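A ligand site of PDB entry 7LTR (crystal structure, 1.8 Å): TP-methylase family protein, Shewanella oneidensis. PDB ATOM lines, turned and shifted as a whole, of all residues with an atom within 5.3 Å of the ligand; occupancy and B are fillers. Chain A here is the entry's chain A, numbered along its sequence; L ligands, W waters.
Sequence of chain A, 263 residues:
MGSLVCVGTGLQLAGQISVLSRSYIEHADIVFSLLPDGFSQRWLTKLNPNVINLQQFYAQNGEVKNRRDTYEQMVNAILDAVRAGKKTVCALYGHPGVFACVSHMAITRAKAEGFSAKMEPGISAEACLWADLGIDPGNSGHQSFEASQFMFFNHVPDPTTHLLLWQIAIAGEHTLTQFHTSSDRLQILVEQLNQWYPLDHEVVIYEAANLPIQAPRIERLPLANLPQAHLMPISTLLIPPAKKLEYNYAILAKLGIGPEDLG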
ATOM      1  N   LEU A  11     -17.092   1.600 -12.375  1.00  0.00           N
ATOM      2  CA  LEU A  11     -16.715   2.440 -11.205  1.00  0.00           C
ATOM      3  C   LEU A  11     -17.569   2.061  -9.985  1.00  0.00           C
ATOM      4  O   LEU A  11     -17.016   1.993  -8.870  1.00  0.00           O
ATOM      5  CB  LEU A  11     -16.883   3.917 -11.560  1.00  0.00           C
ATOM      6  CG  LEU A  11     -15.706   4.546 -12.308  1.00  0.00           C
ATOM      7  CD1 LEU A  11     -14.461   4.566 -11.423  1.00  0.00           C
ATOM      8  CD2 LEU A  11     -15.423   3.819 -13.610  1.00  0.00           C
ATOM      9  N   TYR A  93     -10.697  -1.865 -12.651  1.00  0.00           N
ATOM     10  CA  TYR A  93     -11.810  -0.919 -12.428  1.00  0.00           C
ATOM     11  C   TYR A  93     -11.964  -0.046 -13.691  1.00  0.00           C
ATOM     12  O   TYR A  93     -10.966   0.195 -14.397  1.00  0.00           O
ATOM     13  CB  TYR A  93     -11.589  -0.137 -11.137  1.00  0.00           C
ATOM     14  CG  TYR A  93     -10.640   1.021 -11.238  1.00  0.00           C
ATOM     15  CD1 TYR A  93     -11.074   2.261 -11.692  1.00  0.00           C
ATOM     16  CD2 TYR A  93      -9.310   0.894 -10.888  1.00  0.00           C
ATOM     17  CE1 TYR A  93     -10.207   3.331 -11.792  1.00  0.00           C
ATOM     18  CE2 TYR A  93      -8.433   1.962 -10.977  1.00  0.00           C
ATOM     19  CZ  TYR A  93      -8.885   3.186 -11.436  1.00  0.00           C
ATOM     20  OH  TYR A  93      -8.022   4.246 -11.532  1.00  0.00           O
ATOM     21  N   GLY A  94     -13.207   0.350 -13.986  1.00  0.00           N
ATOM     22  CA  GLY A  94     -13.569   1.162 -15.166  1.00  0.00           C
ATOM     23  C   GLY A  94     -13.519   0.351 -16.450  1.00  0.00           C
ATOM     24  O   GLY A  94     -14.064  -0.781 -16.471  1.00  0.00           O
ATOM     25  N   HIS A  95     -12.922   0.934 -17.494  1.00  0.00           N
ATOM     26  CA  HIS A  95     -12.589   0.299 -18.796  1.00  0.00           C
ATOM     27  C   HIS A  95     -11.128  -0.142 -18.707  1.00  0.00           C
ATOM     28  O   HIS A  95     -10.289   0.659 -18.326  1.00  0.00           O
ATOM     29  CB  HIS A  95     -12.853   1.303 -19.928  1.00  0.00           C
ATOM     30  CG  HIS A  95     -12.704   0.778 -21.322  1.00  0.00           C
ATOM     31  ND1 HIS A  95     -11.590   0.070 -21.751  1.00  0.00           N
ATOM     32  CD2 HIS A  95     -13.500   0.921 -22.408  1.00  0.00           C
ATOM     33  CE1 HIS A  95     -11.726  -0.223 -23.018  1.00  0.00           C
ATOM     34  NE2 HIS A  95     -12.883   0.293 -23.452  1.00  0.00           N
ATOM     35  N   PRO A  96     -10.791  -1.419 -19.006  1.00  0.00           N
ATOM     36  CA  PRO A  96      -9.444  -1.916 -18.766  1.00  0.00           C
ATOM     37  C   PRO A  96      -8.393  -1.354 -19.740  1.00  0.00           C
ATOM     38  O   PRO A  96      -7.219  -1.600 -19.533  1.00  0.00           O
ATOM     39  CB  PRO A  96      -9.583  -3.439 -18.941  1.00  0.00           C
ATOM     40  CG  PRO A  96     -10.746  -3.591 -19.901  1.00  0.00           C
ATOM     41  CD  PRO A  96     -11.666  -2.432 -19.610  1.00  0.00           C
ATOM     42  N   VAL A  98      -8.658   2.089 -20.964  1.00  0.00           N
ATOM     43  CA  VAL A  98      -8.798   3.570 -20.910  1.00  0.00           C
ATOM     44  C   VAL A  98      -7.919   4.119 -19.783  1.00  0.00           C
ATOM     45  O   VAL A  98      -8.191   3.792 -18.608  1.00  0.00           O
ATOM     46  CB  VAL A  98     -10.267   3.998 -20.752  1.00  0.00           C
ATOM     47  CG1 VAL A  98     -10.393   5.473 -20.402  1.00  0.00           C
ATOM     48  CG2 VAL A  98     -11.082   3.677 -22.000  1.00  0.00           C
ATOM     49  N   PHE A  99      -6.922   4.923 -20.138  1.00  0.00           N
ATOM     50  CA  PHE A  99      -5.893   5.473 -19.208  1.00  0.00           C
ATOM     51  C   PHE A  99      -5.396   4.325 -18.313  1.00  0.00           C
ATOM     52  O   PHE A  99      -5.325   4.484 -17.082  1.00  0.00           O
ATOM     53  CB  PHE A  99      -6.456   6.675 -18.463  1.00  0.00           C
ATOM     54  CG  PHE A  99      -6.542   7.930 -19.307  1.00  0.00           C
ATOM     55  CD1 PHE A  99      -7.609   8.127 -20.166  1.00  0.00           C
ATOM     56  CD2 PHE A  99      -5.532   8.876 -19.277  1.00  0.00           C
ATOM     57  CE1 PHE A  99      -7.683   9.266 -20.962  1.00  0.00           C
ATOM     58  CE2 PHE A  99      -5.606  10.015 -20.073  1.00  0.00           C
ATOM     59  CZ  PHE A  99      -6.680  10.201 -20.908  1.00  0.00           C
ATOM     60  N   ALA A 100      -5.063   3.195 -18.956  1.00  0.00           N
ATOM     61  CA  ALA A 100      -4.547   1.953 -18.336  1.00  0.00           C
ATOM     62  C   ALA A 100      -3.679   1.229 -19.359  1.00  0.00           C
ATOM     63  O   ALA A 100      -4.186   0.945 -20.465  1.00  0.00           O
ATOM     64  CB  ALA A 100      -5.697   1.093 -17.881  1.00  0.00           C
ATOM     65  N   ILE A 123     -17.223   0.212 -18.510  1.00  0.00           N
ATOM     66  CA  ILE A 123     -17.728   1.591 -18.269  1.00  0.00           C
ATOM     67  C   ILE A 123     -16.617   2.411 -17.580  1.00  0.00           C
ATOM     68  O   ILE A 123     -16.245   2.076 -16.442  1.00  0.00           O
ATOM     69  CB  ILE A 123     -19.038   1.536 -17.473  1.00  0.00           C
ATOM     70  CG1 ILE A 123     -20.163   0.933 -18.317  1.00  0.00           C
ATOM     71  CG2 ILE A 123     -19.387   2.914 -16.933  1.00  0.00           C
ATOM     72  CD1 ILE A 123     -21.352   0.439 -17.529  1.00  0.00           C
ATOM     73  N   SER A 124     -16.110   3.423 -18.276  1.00  0.00           N
ATOM     74  CA  SER A 124     -14.984   4.298 -17.838  1.00  0.00           C
ATOM     75  C   SER A 124     -15.497   5.443 -16.960  1.00  0.00           C
ATOM     76  O   SER A 124     -16.728   5.683 -16.930  1.00  0.00           O
ATOM     77  CB  SER A 124     -14.241   4.831 -19.030  1.00  0.00           C
ATOM     78  OG  SER A 124     -14.960   5.911 -19.618  1.00  0.00           O
ATOM     79  N   ALA A 125     -14.587   6.139 -16.294  1.00  0.00           N
ATOM     80  CA  ALA A 125     -14.896   7.339 -15.486  1.00  0.00           C
ATOM     81  C   ALA A 125     -15.551   8.396 -16.386  1.00  0.00           C
ATOM     82  O   ALA A 125     -16.468   9.092 -15.899  1.00  0.00           O
ATOM     83  CB  ALA A 125     -13.647   7.861 -14.810  1.00  0.00           C
ATOM     84  N   GLU A 126     -15.122   8.483 -17.648  1.00  0.00           N
ATOM     85  CA  GLU A 126     -15.658   9.439 -18.646  1.00  0.00           C
ATOM     86  C   GLU A 126     -17.120   9.086 -18.957  1.00  0.00           C
ATOM     87  O   GLU A 126     -17.960  10.002 -18.990  1.00  0.00           O
ATOM     88  CB  GLU A 126     -14.806   9.442 -19.920  1.00  0.00           C
ATOM     89  CG  GLU A 126     -15.332  10.381 -20.988  1.00  0.00           C
ATOM     90  CD  GLU A 126     -14.366  10.654 -22.135  1.00  0.00           C
ATOM     91  OE1 GLU A 126     -13.171  10.369 -21.980  1.00  0.00           O
ATOM     92  OE2 GLU A 126     -14.833  11.145 -23.183  1.00  0.00           O
ATOM     93  N   LEU A 165      -8.917  16.522 -18.333  1.00  0.00           N
ATOM     94  CA  LEU A 165      -7.530  16.215 -17.895  1.00  0.00           C
ATOM     95  C   LEU A 165      -7.585  15.117 -16.822  1.00  0.00           C
ATOM     96  O   LEU A 165      -8.109  15.382 -15.736  1.00  0.00           O
ATOM     97  CB  LEU A 165      -6.853  17.485 -17.377  1.00  0.00           C
ATOM     98  CG  LEU A 165      -6.671  18.584 -18.414  1.00  0.00           C
ATOM     99  CD1 LEU A 165      -6.019  19.819 -17.799  1.00  0.00           C
ATOM    100  CD2 LEU A 165      -5.860  18.072 -19.600  1.00  0.00           C
ATOM    101  N   TRP A 166      -7.087  13.928 -17.157  1.00  0.00           N
ATOM    102  CA  TRP A 166      -7.092  12.725 -16.284  1.00  0.00           C
ATOM    103  C   TRP A 166      -5.855  12.758 -15.371  1.00  0.00           C
ATOM    104  O   TRP A 166      -4.859  13.401 -15.757  1.00  0.00           O
ATOM    105  CB  TRP A 166      -7.110  11.443 -17.124  1.00  0.00           C
ATOM    106  CG  TRP A 166      -8.327  11.264 -17.967  1.00  0.00           C
ATOM    107  CD1 TRP A 166      -8.782  12.076 -18.975  1.00  0.00           C
ATOM    108  CD2 TRP A 166      -9.240  10.153 -17.915  1.00  0.00           C
ATOM    109  NE1 TRP A 166      -9.911  11.551 -19.539  1.00  0.00           N
ATOM    110  CE2 TRP A 166     -10.218  10.376 -18.914  1.00  0.00           C
ATOM    111  CE3 TRP A 166      -9.324   9.002 -17.129  1.00  0.00           C
ATOM    112  CZ2 TRP A 166     -11.263   9.485 -19.129  1.00  0.00           C
ATOM    113  CZ3 TRP A 166     -10.365   8.119 -17.347  1.00  0.00           C
ATOM    114  CH2 TRP A 166     -11.325   8.362 -18.332  1.00  0.00           C
ATOM    115  N   GLN A 167      -5.918  12.067 -14.233  1.00  0.00           N
ATOM    116  CA  GLN A 167      -4.806  11.950 -13.254  1.00  0.00           C
ATOM    117  C   GLN A 167      -4.335  13.350 -12.865  1.00  0.00           C
ATOM    118  O   GLN A 167      -3.109  13.578 -12.818  1.00  0.00           O
ATOM    119  CB  GLN A 167      -3.695  11.073 -13.837  1.00  0.00           C
ATOM    120  CG  GLN A 167      -4.172   9.654 -14.125  1.00  0.00           C
ATOM    121  CD  GLN A 167      -3.093   8.725 -14.606  1.00  0.00           C
ATOM    122  OE1 GLN A 167      -1.934   9.101 -14.784  1.00  0.00           O
ATOM    123  NE2 GLN A 167      -3.473   7.473 -14.816  1.00  0.00           N
ATOM    124  N   ILE A 168      -5.280  14.248 -12.560  1.00  0.00           N
ATOM    125  CA  ILE A 168      -5.014  15.688 -12.258  1.00  0.00           C
ATOM    126  C   ILE A 168      -4.244  15.793 -10.927  1.00  0.00           C
ATOM    127  O   ILE A 168      -3.516  16.799 -10.766  1.00  0.00           O
ATOM    128  CB  ILE A 168      -6.335  16.484 -12.240  1.00  0.00           C
ATOM    129  CG1 ILE A 168      -6.086  17.973 -11.985  1.00  0.00           C
ATOM    130  CG2 ILE A 168      -7.320  15.901 -11.241  1.00  0.00           C
ATOM    131  CD1 ILE A 168      -5.430  18.697 -13.142  1.00  0.00           C
ATOM    132  N   TYR A 206     -14.472  16.283 -10.931  1.00  0.00           N
ATOM    133  CA  TYR A 206     -15.441  15.169 -10.991  1.00  0.00           C
ATOM    134  C   TYR A 206     -14.830  13.925 -10.354  1.00  0.00           C
ATOM    135  O   TYR A 206     -13.689  13.555 -10.706  1.00  0.00           O
ATOM    136  CB  TYR A 206     -15.843  14.878 -12.437  1.00  0.00           C
ATOM    137  CG  TYR A 206     -16.777  13.705 -12.553  1.00  0.00           C
ATOM    138  CD1 TYR A 206     -18.057  13.761 -12.027  1.00  0.00           C
ATOM    139  CD2 TYR A 206     -16.371  12.524 -13.150  1.00  0.00           C
ATOM    140  CE1 TYR A 206     -18.911  12.682 -12.104  1.00  0.00           C
ATOM    141  CE2 TYR A 206     -17.221  11.429 -13.233  1.00  0.00           C
ATOM    142  CZ  TYR A 206     -18.499  11.514 -12.717  1.00  0.00           C
ATOM    143  OH  TYR A 206     -19.340  10.439 -12.796  1.00  0.00           O
ATOM    144  N   GLU A 207     -15.581  13.309  -9.440  1.00  0.00           N
ATOM    145  CA  GLU A 207     -15.301  11.948  -8.939  1.00  0.00           C
ATOM    146  C   GLU A 207     -16.591  11.132  -8.998  1.00  0.00           C
ATOM    147  O   GLU A 207     -17.524  11.419  -8.217  1.00  0.00           O
ATOM    148  CB  GLU A 207     -14.721  11.986  -7.523  1.00  0.00           C
ATOM    149  CG  GLU A 207     -13.363  12.656  -7.460  1.00  0.00           C
ATOM    150  CD  GLU A 207     -12.975  13.108  -6.067  1.00  0.00           C
ATOM    151  OE1 GLU A 207     -13.684  12.756  -5.106  1.00  0.00           O
ATOM    152  OE2 GLU A 207     -11.960  13.831  -5.943  1.00  0.00           O
ATOM    153  N   ALA A 208     -16.654  10.183  -9.936  1.00  0.00           N
ATOM    154  CA  ALA A 208     -17.713   9.163 -10.012  1.00  0.00           C
ATOM    155  C   ALA A 208     -17.762   8.420  -8.678  1.00  0.00           C
ATOM    156  O   ALA A 208     -16.687   8.120  -8.133  1.00  0.00           O
ATOM    157  CB  ALA A 208     -17.458   8.223 -11.168  1.00  0.00           C
ATOM    158  N   ALA A 209     -18.968   8.159  -8.166  1.00  0.00           N
ATOM    159  CA  ALA A 209     -19.209   7.348  -6.948  1.00  0.00           C
ATOM    160  C   ALA A 209     -18.778   5.891  -7.212  1.00  0.00           C
ATOM    161  O   ALA A 209     -19.053   5.384  -8.318  1.00  0.00           O
ATOM    162  CB  ALA A 209     -20.665   7.446  -6.565  1.00  0.00           C
ATOM    163  N   ASN A 210     -18.135   5.261  -6.232  1.00  0.00           N
ATOM    164  CA  ASN A 210     -17.720   3.835  -6.295  1.00  0.00           C
ATOM    165  C   ASN A 210     -18.649   2.969  -5.438  1.00  0.00           C
ATOM    166  O   ASN A 210     -18.581   1.740  -5.561  1.00  0.00           O
ATOM    167  CB  ASN A 210     -16.269   3.628  -5.851  1.00  0.00           C
ATOM    168  CG  ASN A 210     -15.254   4.273  -6.766  1.00  0.00           C
ATOM    169  OD1 ASN A 210     -15.154   3.938  -7.946  1.00  0.00           O
ATOM    170  ND2 ASN A 210     -14.454   5.175  -6.216  1.00  0.00           N
ATOM    171  N   PRO A 233      -6.569  10.720  -5.995  1.00  0.00           N
ATOM    172  CA  PRO A 233      -6.124   9.899  -7.124  1.00  0.00           C
ATOM    173  C   PRO A 233      -7.248   9.668  -8.156  1.00  0.00           C
ATOM    174  O   PRO A 233      -6.921   9.515  -9.312  1.00  0.00           O
ATOM    175  CB  PRO A 233      -5.697   8.594  -6.437  1.00  0.00           C
ATOM    176  CG  PRO A 233      -5.238   9.030  -5.064  1.00  0.00           C
ATOM    177  CD  PRO A 233      -6.148  10.181  -4.686  1.00  0.00           C
ATOM    178  N   ILE A 234      -8.513   9.664  -7.716  1.00  0.00           N
ATOM    179  CA  ILE A 234      -9.686   9.329  -8.584  1.00  0.00           C
ATOM    180  C   ILE A 234     -10.241  10.595  -9.252  1.00  0.00           C
ATOM    181  O   ILE A 234     -11.176  10.474 -10.054  1.00  0.00           O
ATOM    182  CB  ILE A 234     -10.785   8.587  -7.791  1.00  0.00           C
ATOM    183  CG1 ILE A 234     -11.443   9.479  -6.738  1.00  0.00           C
ATOM    184  CG2 ILE A 234     -10.255   7.298  -7.188  1.00  0.00           C
ATOM    185  CD1 ILE A 234     -12.811   8.999  -6.305  1.00  0.00           C
ATOM    186  N   SER A 235      -9.685  11.771  -8.929  1.00  0.00           N
ATOM    187  CA  SER A 235     -10.158  13.076  -9.477  1.00  0.00           C
ATOM    188  C   SER A 235      -9.879  13.170 -10.977  1.00  0.00           C
ATOM    189  O   SER A 235      -8.752  12.828 -11.401  1.00  0.00           O
ATOM    190  CB  SER A 235      -9.550  14.239  -8.731  1.00  0.00           C
ATOM    191  OG  SER A 235     -10.024  14.291  -7.398  1.00  0.00           O
ATOM    192  N   THR A 236     -10.874  13.607 -11.750  1.00  0.00           N
ATOM    193  CA  THR A 236     -10.760  14.024 -13.170  1.00  0.00           C
ATOM    194  C   THR A 236     -11.222  15.482 -13.273  1.00  0.00           C
ATOM    195  O   THR A 236     -12.224  15.834 -12.626  1.00  0.00           O
ATOM    196  CB  THR A 236     -11.564  13.104 -14.104  1.00  0.00           C
ATOM    197  OG1 THR A 236     -11.034  11.783 -13.985  1.00  0.00           O
ATOM    198  CG2 THR A 236     -11.523  13.546 -15.549  1.00  0.00           C
HETATM  199  N1  LIG L   1      -9.461   2.582 -16.482  1.00  0.00           N
HETATM  200  C1  LIG L   1     -10.018   3.667 -15.634  1.00  0.00           C
HETATM  201  C2  LIG L   1     -11.330   4.161 -16.265  1.00  0.00           C
HETATM  202  O1  LIG L   1     -11.869   3.517 -17.154  1.00  0.00           O
HETATM  203  O2  LIG L   1     -11.873   5.201 -15.888  1.00  0.00           O
HETATM  204  C3  LIG L   1      -9.037   4.827 -15.495  1.00  0.00           C
HETATM  205  C4  LIG L   1      -7.809   4.486 -14.669  1.00  0.00           C
HETATM  206  S1  LIG L   1      -6.503   5.734 -14.806  1.00  0.00           S
HETATM  207  C5  LIG L   1      -5.073   4.797 -14.298  1.00  0.00           C
HETATM  208  C6  LIG L   1      -6.865   6.702 -13.317  1.00  0.00           C
HETATM  209  C7  LIG L   1      -7.581   7.998 -13.650  1.00  0.00           C
HETATM  210  O3  LIG L   1      -8.939   7.713 -14.062  1.00  0.00           O
HETATM  211  C8  LIG L   1      -7.739   8.987 -12.494  1.00  0.00           C
HETATM  212  O4  LIG L   1      -6.568   9.763 -12.279  1.00  0.00           O
HETATM  213  C9  LIG L   1      -8.905   9.823 -13.013  1.00  0.00           C
HETATM  214  O5  LIG L   1      -8.543  10.766 -13.996  1.00  0.00           O
HETATM  215  C10 LIG L   1      -9.798   8.724 -13.588  1.00  0.00           C
HETATM  216  N2  LIG L   1     -10.708   8.161 -12.600  1.00  0.00           N
HETATM  217  C11 LIG L   1     -10.591   6.964 -11.945  1.00  0.00           C
HETATM  218  N3  LIG L   1     -11.559   6.746 -11.100  1.00  0.00           N
HETATM  219  C12 LIG L   1     -12.371   7.871 -11.192  1.00  0.00           C
HETATM  220  C13 LIG L   1     -13.562   8.241 -10.543  1.00  0.00           C
HETATM  221  N4  LIG L   1     -14.169   7.503  -9.627  1.00  0.00           N
HETATM  222  N5  LIG L   1     -14.103   9.433 -10.881  1.00  0.00           N
HETATM  223  C14 LIG L   1     -13.488  10.188 -11.803  1.00  0.00           C
HETATM  224  N6  LIG L   1     -12.375   9.940 -12.469  1.00  0.00           N
HETATM  225  C15 LIG L   1     -11.851   8.760 -12.123  1.00  0.00           C
HETATM  226  O   HOH W   1     -12.577   4.938  -9.262  1.00  0.00           O
HETATM  227  O   HOH W   2      -8.259   0.699 -14.922  1.00  0.00           O
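A sulfur (S1) of the ligand sits close to the backbone carbonyl oxygen (O) of Phe 99 (2.9 Å).
Residues that only touch the ligand: Tyr 93, Ser 124, Trp 166, Glu 207, Leu 11, Gly 94 and Tyr 206.
Hydrophobic or aromatic side chains that line the ligand: Leu 11, Tyr 93, His 95, Val 98, Phe 99, Ala 125, Trp 166, Tyr 206, Ala 208 and Ile 234.
17 residues have an atom within 4 Å of the ligand: Leu 11, Tyr 93, Gly 94, His 95, Val 98, Phe 99, Ser 124, Ala 125, Trp 166, Gln 167, Tyr 206, Glu 207, Ala 208, Pro 233, Ile 234, Ser 235 and Thr 236.
The backbone NH (N) of Tyr 206 sits at hydrogen-bond distance from the backbone carbonyl oxygen (O) of Thr 236 (2.9 Å).
The side-chain hydroxyl of Ser 124 sits close to the backbone NH of Glu 126, 3.2 Å away.
The side-chain hydroxyl (OG) of Ser 235 sits at hydrogen-bond distance from the side-chain carboxylate (OE2) of Glu 207 (2.5 Å).
The side-chain amide oxygen (OD1) of Asn 210 sits close to the backbone carbonyl oxygen (O) of Leu 11, at 2.8 Å.
Water W2 lies within hydrogen-bond range of a nitrogen (N1) of the ligand and the backbone carbonyl oxygen (O) of Tyr 93.
Water W1 lies within hydrogen-bond range of N3 of the ligand (2.8 Å) and OD1 of Asn 210 (3.1 Å).
An oxygen (O5) of the ligand is in hydrogen-bond range of the side-chain hydroxyl (OG1) of Thr 236 (2.7 Å).
A nitrogen (N6) of the ligand lies close to the backbone carbonyl oxygen of Ile 234.
O of Val 98 is in hydrogen-bond range of N1 of the ligand (2.8 Å).
N of His 95 is in hydrogen-bond range of O1 of the ligand (2.8 Å).
The backbone carbonyl oxygen (O) of His 95 is in hydrogen-bond range of a nitrogen (N1) of the ligand (2.8 Å).
The backbone NH (N) of Ala 208 sits at hydrogen-bond distance from a nitrogen (N5) of the ligand (2.8 Å).
The backbone carbonyl oxygen of Ala 208 is in hydrogen-bond range of a nitrogen (N4) of the ligand (3.0 Å).
N of Ala 125 is in hydrogen-bond range of O2 of the ligand, at 2.9 Å.
N of Gln 167 is in hydrogen-bond range of O5 of the ligand.
O4 of the ligand lies within hydrogen-bond range of O of Pro 233, 3.0 Å away.
The backbone carbonyl oxygen (O) of Ser 235 is in hydrogen-bond range of an oxygen (O5) of the ligand, at 3.3 Å.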
